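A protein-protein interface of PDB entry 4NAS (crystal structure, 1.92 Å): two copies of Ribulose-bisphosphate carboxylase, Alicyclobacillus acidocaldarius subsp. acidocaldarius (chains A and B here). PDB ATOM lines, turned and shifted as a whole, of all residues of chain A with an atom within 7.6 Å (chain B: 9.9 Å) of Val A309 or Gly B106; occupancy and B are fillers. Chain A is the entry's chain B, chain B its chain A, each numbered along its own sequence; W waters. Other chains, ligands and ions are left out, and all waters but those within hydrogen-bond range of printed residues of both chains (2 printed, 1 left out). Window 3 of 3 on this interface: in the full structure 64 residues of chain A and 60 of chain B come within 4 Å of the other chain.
OG of Ser B103 is in hydrogen-bond range of N of Gly A272 (3.1 Å). The side-chain sulfur of Met B104 lies close to the side-chain hydroxyl of Tyr A275, at 3.7 Å.
Of chain B, only Met B104 (3.8 Å) and Gly B106 (3.8 Å) come within 4 Å of Val A309. Of the printed residues of chain A, Gly B106 touches Val A309 (3.8 Å). Of the printed residues of chain B, Gly A272 touches Ser B103 (3.1 Å) and Met B104 (3.6 Å). Printed residues of chain A within 4 Å of Ser B277: Ser A277. Printed residues of chain B within 4 Å of Tyr A275: Met B104. Of the printed residues of chain A, Ser B103 touches Gly A272. Of the printed residues of chain A, Met B104 touches Gly A272, Tyr A275 and Val A309. Asn B279 touches none of the printed residues of chain A. Leu B19 touches none of the printed residues of chain A. The nearest residue of chain A that does not touch Gly B106 is Gly A276 (5.6 Å).
Gly A272 touches Met B104 (N to CG, 3.6 Å). CE2 of Tyr B280 touches O of Gly A276 (3.4 Å). CB of Ser A277 touches CB of Ser B277, at 3.6 Å. CA of Ser A277 touches CD1 of Tyr B280 (3.6 Å). Val A309 touches Met B104. CG1 of Val A309 touches N of Gly B106, at 3.8 Å.
Of the 23 printed residues of chain B, 5 touch a printed residue of chain A. Among the printed residues, 8 pairs touch across the chains.
The backbone carbonyl oxygen (O) of Tyr B280 is in hydrogen-bond range of the guanidinium group (NE) of Arg B109 (3.1 Å). The side-chain hydroxyl of Ser B103 is in hydrogen-bond range of the backbone carbonyl oxygen of Gly B100, 2.8 Å away. The guanidinium group of Arg B109 lies within hydrogen-bond range of the backbone carbonyl oxygen of Ser B277 (3.3 Å). The backbone NH (N) of Tyr B280 sits at hydrogen-bond distance from the side-chain hydroxyl (OG) of Ser B277 (3.1 Å).
Ser B277 touches its own counterpart, Ser A277.
Water W2 bridges the backbone carbonyl oxygen (O) of Val A309 (2.4 Å) and the backbone carbonyl oxygen (O) of Met B104 (3.2 Å). Water W1 lies within hydrogen-bond range of OH of Tyr A275 (2.8 Å) and O of Met B104 (3.1 Å).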
ATOM      1  N   GLY A 272      -1.437  10.430  14.172  1.00  0.00           N
ATOM      2  CA  GLY A 272      -0.918  11.423  15.100  1.00  0.00           C
ATOM      3  C   GLY A 272      -0.312  10.841  16.356  1.00  0.00           C
ATOM      4  O   GLY A 272       0.472  11.501  17.039  1.00  0.00           O
ATOM      5  N   TYR A 275       3.329  10.628  15.137  1.00  0.00           N
ATOM      6  CA  TYR A 275       4.109  11.790  14.695  1.00  0.00           C
ATOM      7  C   TYR A 275       3.931  13.075  15.503  1.00  0.00           C
ATOM      8  O   TYR A 275       4.671  14.043  15.314  1.00  0.00           O
ATOM      9  CB  TYR A 275       3.862  12.046  13.205  1.00  0.00           C
ATOM     10  CG  TYR A 275       2.498  12.646  12.888  1.00  0.00           C
ATOM     11  CD1 TYR A 275       2.197  13.945  13.273  1.00  0.00           C
ATOM     12  CD2 TYR A 275       1.530  11.930  12.184  1.00  0.00           C
ATOM     13  CE1 TYR A 275       0.973  14.506  13.027  1.00  0.00           C
ATOM     14  CE2 TYR A 275       0.296  12.508  11.901  1.00  0.00           C
ATOM     15  CZ  TYR A 275       0.039  13.801  12.339  1.00  0.00           C
ATOM     16  OH  TYR A 275      -1.140  14.448  12.105  1.00  0.00           O
ATOM     17  N   GLY A 276       2.942  13.092  16.385  1.00  0.00           N
ATOM     18  CA  GLY A 276       2.564  14.301  17.096  1.00  0.00           C
ATOM     19  C   GLY A 276       3.662  14.973  17.896  1.00  0.00           C
ATOM     20  O   GLY A 276       3.783  16.207  17.930  1.00  0.00           O
ATOM     21  N   SER A 277       4.475  14.156  18.543  1.00  0.00           N
ATOM     22  CA  SER A 277       5.546  14.677  19.362  1.00  0.00           C
ATOM     23  C   SER A 277       6.719  15.136  18.493  1.00  0.00           C
ATOM     24  O   SER A 277       7.064  14.489  17.510  1.00  0.00           O
ATOM     25  CB  SER A 277       6.023  13.605  20.332  1.00  0.00           C
ATOM     26  OG  SER A 277       7.397  13.774  20.610  1.00  0.00           O
ATOM     27  N   PRO A 303      -3.316  16.325   7.323  1.00  0.00           N
ATOM     28  CA  PRO A 303      -3.695  17.658   7.824  1.00  0.00           C
ATOM     29  C   PRO A 303      -3.113  18.775   6.968  1.00  0.00           C
ATOM     30  O   PRO A 303      -1.915  18.697   6.666  1.00  0.00           O
ATOM     31  CB  PRO A 303      -3.062  17.690   9.230  1.00  0.00           C
ATOM     32  CG  PRO A 303      -2.994  16.288   9.634  1.00  0.00           C
ATOM     33  CD  PRO A 303      -2.755  15.479   8.395  1.00  0.00           C
ATOM     34  N   SER A 304      -3.929  19.760   6.566  1.00  0.00           N
ATOM     35  CA  SER A 304      -3.459  20.880   5.734  1.00  0.00           C
ATOM     36  C   SER A 304      -2.679  21.892   6.562  1.00  0.00           C
ATOM     37  O   SER A 304      -2.721  21.857   7.792  1.00  0.00           O
ATOM     38  CB  SER A 304      -4.617  21.636   5.079  1.00  0.00           C
ATOM     39  OG  SER A 304      -5.276  22.478   6.036  1.00  0.00           O
ATOM     40  N   MET A 305      -2.016  22.825   5.872  1.00  0.00           N
ATOM     41  CA  MET A 305      -1.280  23.886   6.530  1.00  0.00           C
ATOM     42  C   MET A 305      -2.251  24.975   6.946  1.00  0.00           C
ATOM     43  O   MET A 305      -1.827  26.004   7.468  1.00  0.00           O
ATOM     44  CB  MET A 305      -0.221  24.471   5.593  1.00  0.00           C
ATOM     45  CG  MET A 305       1.042  23.635   5.463  1.00  0.00           C
ATOM     46  SD  MET A 305       1.987  23.601   7.162  1.00  0.00           S
ATOM     47  CE  MET A 305       2.912  25.315   6.996  1.00  0.00           C
ATOM     48  N   TYR A 306      -3.544  24.734   6.732  1.00  0.00           N
ATOM     49  CA  TYR A 306      -4.585  25.752   6.949  1.00  0.00           C
ATOM     50  C   TYR A 306      -5.540  25.473   8.134  1.00  0.00           C
ATOM     51  O   TYR A 306      -6.433  26.277   8.445  1.00  0.00           O
ATOM     52  CB  TYR A 306      -5.333  26.012   5.616  1.00  0.00           C
ATOM     53  CG  TYR A 306      -4.346  26.467   4.548  1.00  0.00           C
ATOM     54  CD1 TYR A 306      -3.747  27.715   4.627  1.00  0.00           C
ATOM     55  CD2 TYR A 306      -3.939  25.616   3.530  1.00  0.00           C
ATOM     56  CE1 TYR A 306      -2.803  28.131   3.692  1.00  0.00           C
ATOM     57  CE2 TYR A 306      -2.993  26.015   2.591  1.00  0.00           C
ATOM     58  CZ  TYR A 306      -2.431  27.280   2.680  1.00  0.00           C
ATOM     59  OH  TYR A 306      -1.496  27.701   1.759  1.00  0.00           O
ATOM     60  N   GLY A 307      -5.357  24.348   8.808  1.00  0.00           N
ATOM     61  CA  GLY A 307      -6.173  24.018   9.972  1.00  0.00           C
ATOM     62  C   GLY A 307      -5.526  24.477  11.270  1.00  0.00           C
ATOM     63  O   GLY A 307      -4.472  25.108  11.246  1.00  0.00           O
ATOM     64  N   SER A 308      -6.146  24.150  12.402  1.00  0.00           N
ATOM     65  CA  SER A 308      -5.689  24.623  13.711  1.00  0.00           C
ATOM     66  C   SER A 308      -4.329  24.052  14.085  1.00  0.00           C
ATOM     67  O   SER A 308      -3.501  24.722  14.702  1.00  0.00           O
ATOM     68  CB  SER A 308      -6.702  24.245  14.799  1.00  0.00           C
ATOM     69  OG  SER A 308      -7.988  24.750  14.507  1.00  0.00           O
ATOM     70  N   VAL A 309      -4.123  22.797  13.715  1.00  0.00           N
ATOM     71  CA  VAL A 309      -2.890  22.093  13.996  1.00  0.00           C
ATOM     72  C   VAL A 309      -2.377  21.538  12.672  1.00  0.00           C
ATOM     73  O   VAL A 309      -3.058  20.744  12.026  1.00  0.00           O
ATOM     74  CB  VAL A 309      -3.138  20.934  14.975  1.00  0.00           C
ATOM     75  CG1 VAL A 309      -1.860  20.111  15.169  1.00  0.00           C
ATOM     76  CG2 VAL A 309      -3.702  21.460  16.306  1.00  0.00           C
ATOM     77  N   THR A 310      -1.193  21.975  12.257  1.00  0.00           N
ATOM     78  CA  THR A 310      -0.652  21.549  10.969  1.00  0.00           C
ATOM     79  C   THR A 310       0.449  20.509  11.188  1.00  0.00           C
ATOM     80  O   THR A 310       0.723  20.097  12.321  1.00  0.00           O
ATOM     81  CB  THR A 310      -0.088  22.733  10.156  1.00  0.00           C
ATOM     82  OG1 THR A 310       1.188  23.108  10.695  1.00  0.00           O
ATOM     83  CG2 THR A 310      -1.020  23.933  10.228  1.00  0.00           C
ATOM     84  N   LEU A 311       1.068  20.075  10.105  1.00  0.00           N
ATOM     85  CA  LEU A 311       2.216  19.181  10.221  1.00  0.00           C
ATOM     86  C   LEU A 311       3.463  20.028  10.307  1.00  0.00           C
ATOM     87  O   LEU A 311       4.537  19.521  10.607  1.00  0.00           O
ATOM     88  CB  LEU A 311       2.306  18.254   9.006  1.00  0.00           C
ATOM     89  CG  LEU A 311       1.211  17.189   8.856  1.00  0.00           C
ATOM     90  CD1 LEU A 311       1.522  16.293   7.667  1.00  0.00           C
ATOM     91  CD2 LEU A 311       0.997  16.345  10.125  1.00  0.00           C
ATOM     92  N   GLY A 312       3.314  21.327  10.048  1.00  0.00           N
ATOM     93  CA  GLY A 312       4.466  22.182   9.835  1.00  0.00           C
ATOM     94  C   GLY A 312       4.958  22.159   8.396  1.00  0.00           C
ATOM     95  O   GLY A 312       4.837  21.148   7.682  1.00  0.00           O
ATOM     96  N   SER A 337      -6.615  18.264   4.516  1.00  0.00           N
ATOM     97  CA  SER A 337      -7.852  18.399   5.261  1.00  0.00           C
ATOM     98  C   SER A 337      -7.771  19.574   6.237  1.00  0.00           C
ATOM     99  O   SER A 337      -6.667  19.980   6.639  1.00  0.00           O
ATOM    100  CB  SER A 337      -8.158  17.094   6.015  1.00  0.00           C
ATOM    101  OG  SER A 337      -7.191  16.826   7.035  1.00  0.00           O
ATOM    102  N   ALA A 338      -8.946  20.096   6.601  1.00  0.00           N
ATOM    103  CA  ALA A 338      -9.122  21.231   7.530  1.00  0.00           C
ATOM    104  C   ALA A 338      -8.863  22.624   6.941  1.00  0.00           C
ATOM    105  O   ALA A 338      -7.861  22.866   6.277  1.00  0.00           O
ATOM    106  CB  ALA A 338      -8.356  21.030   8.845  1.00  0.00           C
ATOM    107  N   TYR B  17      -8.314  11.300  28.329  1.00  0.00           N
ATOM    108  CA  TYR B  17      -7.298  11.971  27.533  1.00  0.00           C
ATOM    109  C   TYR B  17      -6.617  12.994  28.413  1.00  0.00           C
ATOM    110  O   TYR B  17      -7.292  13.694  29.156  1.00  0.00           O
ATOM    111  CB  TYR B  17      -7.946  12.711  26.362  1.00  0.00           C
ATOM    112  CG  TYR B  17      -8.758  11.817  25.464  1.00  0.00           C
ATOM    113  CD1 TYR B  17      -8.137  11.010  24.544  1.00  0.00           C
ATOM    114  CD2 TYR B  17     -10.147  11.789  25.538  1.00  0.00           C
ATOM    115  CE1 TYR B  17      -8.861  10.167  23.725  1.00  0.00           C
ATOM    116  CE2 TYR B  17     -10.889  10.955  24.718  1.00  0.00           C
ATOM    117  CZ  TYR B  17     -10.226  10.131  23.819  1.00  0.00           C
ATOM    118  OH  TYR B  17     -10.925   9.288  22.985  1.00  0.00           O
ATOM    119  N   ARG B  18      -5.290  13.068  28.339  1.00  0.00           N
ATOM    120  CA  ARG B  18      -4.560  14.212  28.876  1.00  0.00           C
ATOM    121  C   ARG B  18      -4.292  15.165  27.720  1.00  0.00           C
ATOM    122  O   ARG B  18      -3.789  14.763  26.678  1.00  0.00           O
ATOM    123  CB  ARG B  18      -3.226  13.783  29.485  1.00  0.00           C
ATOM    124  CG  ARG B  18      -2.300  14.967  29.804  1.00  0.00           C
ATOM    125  CD  ARG B  18      -0.821  14.602  29.693  1.00  0.00           C
ATOM    126  NE  ARG B  18       0.054  15.619  30.288  1.00  0.00           N
ATOM    127  CZ  ARG B  18       0.514  16.702  29.656  1.00  0.00           C
ATOM    128  NH1 ARG B  18       0.185  16.962  28.388  1.00  0.00           N
ATOM    129  NH2 ARG B  18       1.310  17.541  30.297  1.00  0.00           N
ATOM    130  N   LEU B  19      -4.608  16.437  27.909  1.00  0.00           N
ATOM    131  CA  LEU B  19      -4.482  17.392  26.826  1.00  0.00           C
ATOM    132  C   LEU B  19      -4.206  18.797  27.345  1.00  0.00           C
ATOM    133  O   LEU B  19      -4.380  19.080  28.534  1.00  0.00           O
ATOM    134  CB  LEU B  19      -5.725  17.375  25.918  1.00  0.00           C
ATOM    135  CG  LEU B  19      -7.131  17.529  26.517  1.00  0.00           C
ATOM    136  CD1 LEU B  19      -7.446  18.947  26.862  1.00  0.00           C
ATOM    137  CD2 LEU B  19      -8.157  17.002  25.531  1.00  0.00           C
ATOM    138  N   ARG B  20      -3.759  19.662  26.443  1.00  0.00           N
ATOM    139  CA  ARG B  20      -3.517  21.050  26.779  1.00  0.00           C
ATOM    140  C   ARG B  20      -4.461  21.931  25.983  1.00  0.00           C
ATOM    141  O   ARG B  20      -4.571  21.789  24.766  1.00  0.00           O
ATOM    142  CB  ARG B  20      -2.068  21.433  26.476  1.00  0.00           C
ATOM    143  CG  ARG B  20      -1.736  22.894  26.773  1.00  0.00           C
ATOM    144  CD  ARG B  20      -0.236  23.110  26.895  1.00  0.00           C
ATOM    145  NE  ARG B  20       0.063  24.468  27.331  1.00  0.00           N
ATOM    146  CZ  ARG B  20       1.221  24.851  27.864  1.00  0.00           C
ATOM    147  NH1 ARG B  20       2.203  23.970  28.037  1.00  0.00           N
ATOM    148  NH2 ARG B  20       1.393  26.118  28.234  1.00  0.00           N
ATOM    149  N   ASP B  21      -5.134  22.848  26.669  1.00  0.00           N
ATOM    150  CA  ASP B  21      -6.027  23.788  25.999  1.00  0.00           C
ATOM    151  C   ASP B  21      -6.254  25.012  26.881  1.00  0.00           C
ATOM    152  O   ASP B  21      -5.815  25.045  28.033  1.00  0.00           O
ATOM    153  CB  ASP B  21      -7.361  23.110  25.687  1.00  0.00           C
ATOM    154  CG  ASP B  21      -8.018  23.647  24.421  1.00  0.00           C
ATOM    155  OD1 ASP B  21      -7.314  23.865  23.411  1.00  0.00           O
ATOM    156  OD2 ASP B  21      -9.249  23.845  24.434  1.00  0.00           O
ATOM    157  N   ARG B  22      -6.932  26.020  26.341  1.00  0.00           N
ATOM    158  CA  ARG B  22      -7.368  27.149  27.153  1.00  0.00           C
ATOM    159  C   ARG B  22      -8.434  26.671  28.126  1.00  0.00           C
ATOM    160  O   ARG B  22      -9.257  25.817  27.785  1.00  0.00           O
ATOM    161  CB  ARG B  22      -7.898  28.287  26.282  1.00  0.00           C
ATOM    162  CG  ARG B  22      -6.831  29.292  25.858  1.00  0.00           C
ATOM    163  CD  ARG B  22      -7.007  29.730  24.404  1.00  0.00           C
ATOM    164  NE  ARG B  22      -6.538  28.717  23.458  1.00  0.00           N
ATOM    165  CZ  ARG B  22      -6.647  28.818  22.135  1.00  0.00           C
ATOM    166  NH1 ARG B  22      -7.219  29.886  21.596  1.00  0.00           N
ATOM    167  NH2 ARG B  22      -6.189  27.850  21.351  1.00  0.00           N
ATOM    168  N   ARG B  29     -14.810  21.934  23.927  1.00  0.00           N
ATOM    169  CA  ARG B  29     -14.020  20.945  23.213  1.00  0.00           C
ATOM    170  C   ARG B  29     -14.461  19.533  23.565  1.00  0.00           C
ATOM    171  O   ARG B  29     -14.589  18.677  22.691  1.00  0.00           O
ATOM    172  CB  ARG B  29     -12.536  21.144  23.457  1.00  0.00           C
ATOM    173  CG  ARG B  29     -11.700  20.300  22.529  1.00  0.00           C
ATOM    174  CD  ARG B  29     -10.247  20.566  22.717  1.00  0.00           C
ATOM    175  NE  ARG B  29      -9.443  19.575  22.009  1.00  0.00           N
ATOM    176  CZ  ARG B  29      -8.128  19.484  22.120  1.00  0.00           C
ATOM    177  NH1 ARG B  29      -7.477  20.336  22.908  1.00  0.00           N
ATOM    178  NH2 ARG B  29      -7.467  18.549  21.444  1.00  0.00           N
ATOM    179  N   PHE B  99      -9.228   7.319  19.236  1.00  0.00           N
ATOM    180  CA  PHE B  99      -7.966   8.023  18.976  1.00  0.00           C
ATOM    181  C   PHE B  99      -7.551   7.995  17.514  1.00  0.00           C
ATOM    182  O   PHE B  99      -6.391   7.786  17.203  1.00  0.00           O
ATOM    183  CB  PHE B  99      -6.845   7.491  19.882  1.00  0.00           C
ATOM    184  CG  PHE B  99      -5.878   8.572  20.348  1.00  0.00           C
ATOM    185  CD1 PHE B  99      -6.341   9.711  20.987  1.00  0.00           C
ATOM    186  CD2 PHE B  99      -4.528   8.447  20.147  1.00  0.00           C
ATOM    187  CE1 PHE B  99      -5.464  10.714  21.428  1.00  0.00           C
ATOM    188  CE2 PHE B  99      -3.631   9.446  20.605  1.00  0.00           C
ATOM    189  CZ  PHE B  99      -4.112  10.579  21.226  1.00  0.00           C
ATOM    190  N   GLY B 100      -8.513   8.232  16.626  1.00  0.00           N
ATOM    191  CA  GLY B 100      -8.259   8.307  15.195  1.00  0.00           C
ATOM    192  C   GLY B 100      -7.985   9.746  14.797  1.00  0.00           C
ATOM    193  O   GLY B 100      -6.833  10.186  14.814  1.00  0.00           O
ATOM    194  N   LYS B 101      -9.040  10.491  14.472  1.00  0.00           N
ATOM    195  CA  LYS B 101      -8.896  11.918  14.165  1.00  0.00           C
ATOM    196  C   LYS B 101      -8.390  12.694  15.376  1.00  0.00           C
ATOM    197  O   LYS B 101      -7.646  13.669  15.239  1.00  0.00           O
ATOM    198  CB  LYS B 101     -10.212  12.512  13.677  1.00  0.00           C
ATOM    199  N   LEU B 102      -8.767  12.236  16.562  1.00  0.00           N
ATOM    200  CA  LEU B 102      -8.372  12.900  17.802  1.00  0.00           C
ATOM    201  C   LEU B 102      -6.848  12.878  18.030  1.00  0.00           C
ATOM    202  O   LEU B 102      -6.295  13.803  18.611  1.00  0.00           O
ATOM    203  CB  LEU B 102      -9.116  12.274  18.988  1.00  0.00           C
ATOM    204  CG  LEU B 102      -9.234  13.033  20.304  1.00  0.00           C
ATOM    205  CD1 LEU B 102      -9.598  14.510  20.110  1.00  0.00           C
ATOM    206  CD2 LEU B 102     -10.304  12.347  21.174  1.00  0.00           C
ATOM    207  N   SER B 103      -6.178  11.826  17.562  1.00  0.00           N
ATOM    208  CA  SER B 103      -4.738  11.658  17.763  1.00  0.00           C
ATOM    209  C   SER B 103      -3.939  12.807  17.141  1.00  0.00           C
ATOM    210  O   SER B 103      -2.815  13.081  17.541  1.00  0.00           O
ATOM    211  CB  SER B 103      -4.263  10.328  17.143  1.00  0.00           C
ATOM    212  OG  SER B 103      -4.171  10.430  15.717  1.00  0.00           O
ATOM    213  N   MET B 104      -4.524  13.452  16.146  1.00  0.00           N
ATOM    214  CA  MET B 104      -3.879  14.544  15.416  1.00  0.00           C
ATOM    215  C   MET B 104      -4.287  15.946  15.899  1.00  0.00           C
ATOM    216  O   MET B 104      -3.996  16.942  15.241  1.00  0.00           O
ATOM    217  CB  MET B 104      -4.229  14.421  13.937  1.00  0.00           C
ATOM    218  CG  MET B 104      -3.660  13.166  13.293  1.00  0.00           C
ATOM    219  SD  MET B 104      -4.507  12.933  11.530  1.00  0.00           S
ATOM    220  CE  MET B 104      -6.077  12.028  12.127  1.00  0.00           C
ATOM    221  N   ASP B 105      -4.963  16.043  17.038  1.00  0.00           N
ATOM    222  CA  ASP B 105      -5.410  17.372  17.487  1.00  0.00           C
ATOM    223  C   ASP B 105      -4.417  18.023  18.468  1.00  0.00           C
ATOM    224  O   ASP B 105      -4.798  18.402  19.570  1.00  0.00           O
ATOM    225  CB  ASP B 105      -6.785  17.274  18.144  1.00  0.00           C
ATOM    226  CG  ASP B 105      -7.903  17.032  17.135  1.00  0.00           C
ATOM    227  OD1 ASP B 105      -7.741  17.430  15.955  1.00  0.00           O
ATOM    228  OD2 ASP B 105      -8.947  16.450  17.527  1.00  0.00           O
ATOM    229  N   GLY B 106      -3.141  18.115  18.092  1.00  0.00           N
ATOM    230  CA  GLY B 106      -2.166  18.778  18.950  1.00  0.00           C
ATOM    231  C   GLY B 106      -1.699  17.954  20.147  1.00  0.00           C
ATOM    232  O   GLY B 106      -1.533  16.726  20.058  1.00  0.00           O
ATOM    233  N   GLU B 107      -1.451  18.630  21.268  1.00  0.00           N
ATOM    234  CA  GLU B 107      -0.984  17.962  22.480  1.00  0.00           C
ATOM    235  C   GLU B 107      -2.144  17.238  23.159  1.00  0.00           C
ATOM    236  O   GLU B 107      -2.967  17.854  23.836  1.00  0.00           O
ATOM    237  CB  GLU B 107      -0.300  18.964  23.436  1.00  0.00           C
ATOM    238  CG  GLU B 107       0.495  18.296  24.585  1.00  0.00           C
ATOM    239  CD  GLU B 107       1.123  19.290  25.554  1.00  0.00           C
ATOM    240  OE1 GLU B 107       1.566  20.375  25.113  1.00  0.00           O
ATOM    241  OE2 GLU B 107       1.159  18.985  26.770  1.00  0.00           O
ATOM    242  N   ILE B 108      -2.232  15.930  22.925  1.00  0.00           N
ATOM    243  CA  ILE B 108      -3.268  15.104  23.532  1.00  0.00           C
ATOM    244  C   ILE B 108      -2.758  13.677  23.555  1.00  0.00           C
ATOM    245  O   ILE B 108      -2.092  13.248  22.632  1.00  0.00           O
ATOM    246  CB  ILE B 108      -4.587  15.180  22.755  1.00  0.00           C
ATOM    247  CG1 ILE B 108      -5.664  14.275  23.383  1.00  0.00           C
ATOM    248  CG2 ILE B 108      -4.382  14.854  21.279  1.00  0.00           C
ATOM    249  CD1 ILE B 108      -7.033  14.508  22.770  1.00  0.00           C
ATOM    250  N   ARG B 109      -3.077  12.952  24.614  1.00  0.00           N
ATOM    251  CA  ARG B 109      -2.540  11.624  24.805  1.00  0.00           C
ATOM    252  C   ARG B 109      -3.615  10.731  25.399  1.00  0.00           C
ATOM    253  O   ARG B 109      -4.294  11.117  26.346  1.00  0.00           O
ATOM    254  CB  ARG B 109      -1.325  11.691  25.744  1.00  0.00           C
ATOM    255  CG  ARG B 109      -0.564  10.356  25.923  1.00  0.00           C
ATOM    256  CD  ARG B 109       0.530  10.492  26.985  1.00  0.00           C
ATOM    257  NE  ARG B 109       1.669   9.595  26.783  1.00  0.00           N
ATOM    258  CZ  ARG B 109       1.909   8.521  27.523  1.00  0.00           C
ATOM    259  NH1 ARG B 109       1.080   8.220  28.505  1.00  0.00           N
ATOM    260  NH2 ARG B 109       2.986   7.765  27.303  1.00  0.00           N
ATOM    261  N   LEU B 110      -3.759   9.527  24.864  1.00  0.00           N
ATOM    262  CA  LEU B 110      -4.705   8.554  25.422  1.00  0.00           C
ATOM    263  C   LEU B 110      -4.142   7.826  26.647  1.00  0.00           C
ATOM    264  O   LEU B 110      -3.187   7.044  26.529  1.00  0.00           O
ATOM    265  CB  LEU B 110      -5.106   7.538  24.337  1.00  0.00           C
ATOM    266  CG  LEU B 110      -6.025   6.391  24.781  1.00  0.00           C
ATOM    267  CD1 LEU B 110      -7.386   6.934  25.308  1.00  0.00           C
ATOM    268  CD2 LEU B 110      -6.243   5.394  23.647  1.00  0.00           C
ATOM    269  N   SER B 277       6.760   9.484  24.104  1.00  0.00           N
ATOM    270  CA  SER B 277       6.630  10.861  24.559  1.00  0.00           C
ATOM    271  C   SER B 277       5.678  10.953  25.743  1.00  0.00           C
ATOM    272  O   SER B 277       4.707  10.230  25.800  1.00  0.00           O
ATOM    273  CB  SER B 277       6.107  11.749  23.434  1.00  0.00           C
ATOM    274  OG  SER B 277       4.713  11.630  23.318  1.00  0.00           O
ATOM    275  N   ASN B 279       3.708  13.527  26.402  1.00  0.00           N
ATOM    276  CA  ASN B 279       2.560  14.403  26.125  1.00  0.00           C
ATOM    277  C   ASN B 279       1.694  14.051  24.912  1.00  0.00           C
ATOM    278  O   ASN B 279       0.667  14.738  24.647  1.00  0.00           O
ATOM    279  CB  ASN B 279       3.047  15.844  25.988  1.00  0.00           C
ATOM    280  CG  ASN B 279       3.773  16.316  27.218  1.00  0.00           C
ATOM    281  OD1 ASN B 279       3.447  15.910  28.328  1.00  0.00           O
ATOM    282  ND2 ASN B 279       4.780  17.158  27.030  1.00  0.00           N
ATOM    283  N   TYR B 280       2.115  13.016  24.175  1.00  0.00           N
ATOM    284  CA  TYR B 280       1.457  12.573  22.941  1.00  0.00           C
ATOM    285  C   TYR B 280       1.285  11.065  22.920  1.00  0.00           C
ATOM    286  O   TYR B 280       1.799  10.390  23.797  1.00  0.00           O
ATOM    287  CB  TYR B 280       2.267  12.999  21.706  1.00  0.00           C
ATOM    288  CG  TYR B 280       2.379  14.509  21.513  1.00  0.00           C
ATOM    289  CD1 TYR B 280       3.374  15.248  22.161  1.00  0.00           C
ATOM    290  CD2 TYR B 280       1.492  15.193  20.682  1.00  0.00           C
ATOM    291  CE1 TYR B 280       3.478  16.620  21.998  1.00  0.00           C
ATOM    292  CE2 TYR B 280       1.593  16.579  20.505  1.00  0.00           C
ATOM    293  CZ  TYR B 280       2.587  17.282  21.169  1.00  0.00           C
ATOM    294  OH  TYR B 280       2.700  18.640  20.986  1.00  0.00           O
ATOM    295  N   GLY B 281       0.553  10.539  21.931  1.00  0.00           N
ATOM    296  CA  GLY B 281       0.427   9.103  21.754  1.00  0.00           C
ATOM    297  C   GLY B 281      -0.495   8.381  22.727  1.00  0.00           C
ATOM    298  O   GLY B 281      -1.509   8.933  23.178  1.00  0.00           O
HETATM  299  O   HOH W   1      -1.535  16.907  13.356  1.00  0.00           O
HETATM  300  O   HOH W   2      -3.731  18.468  12.485  1.00  0.00           O
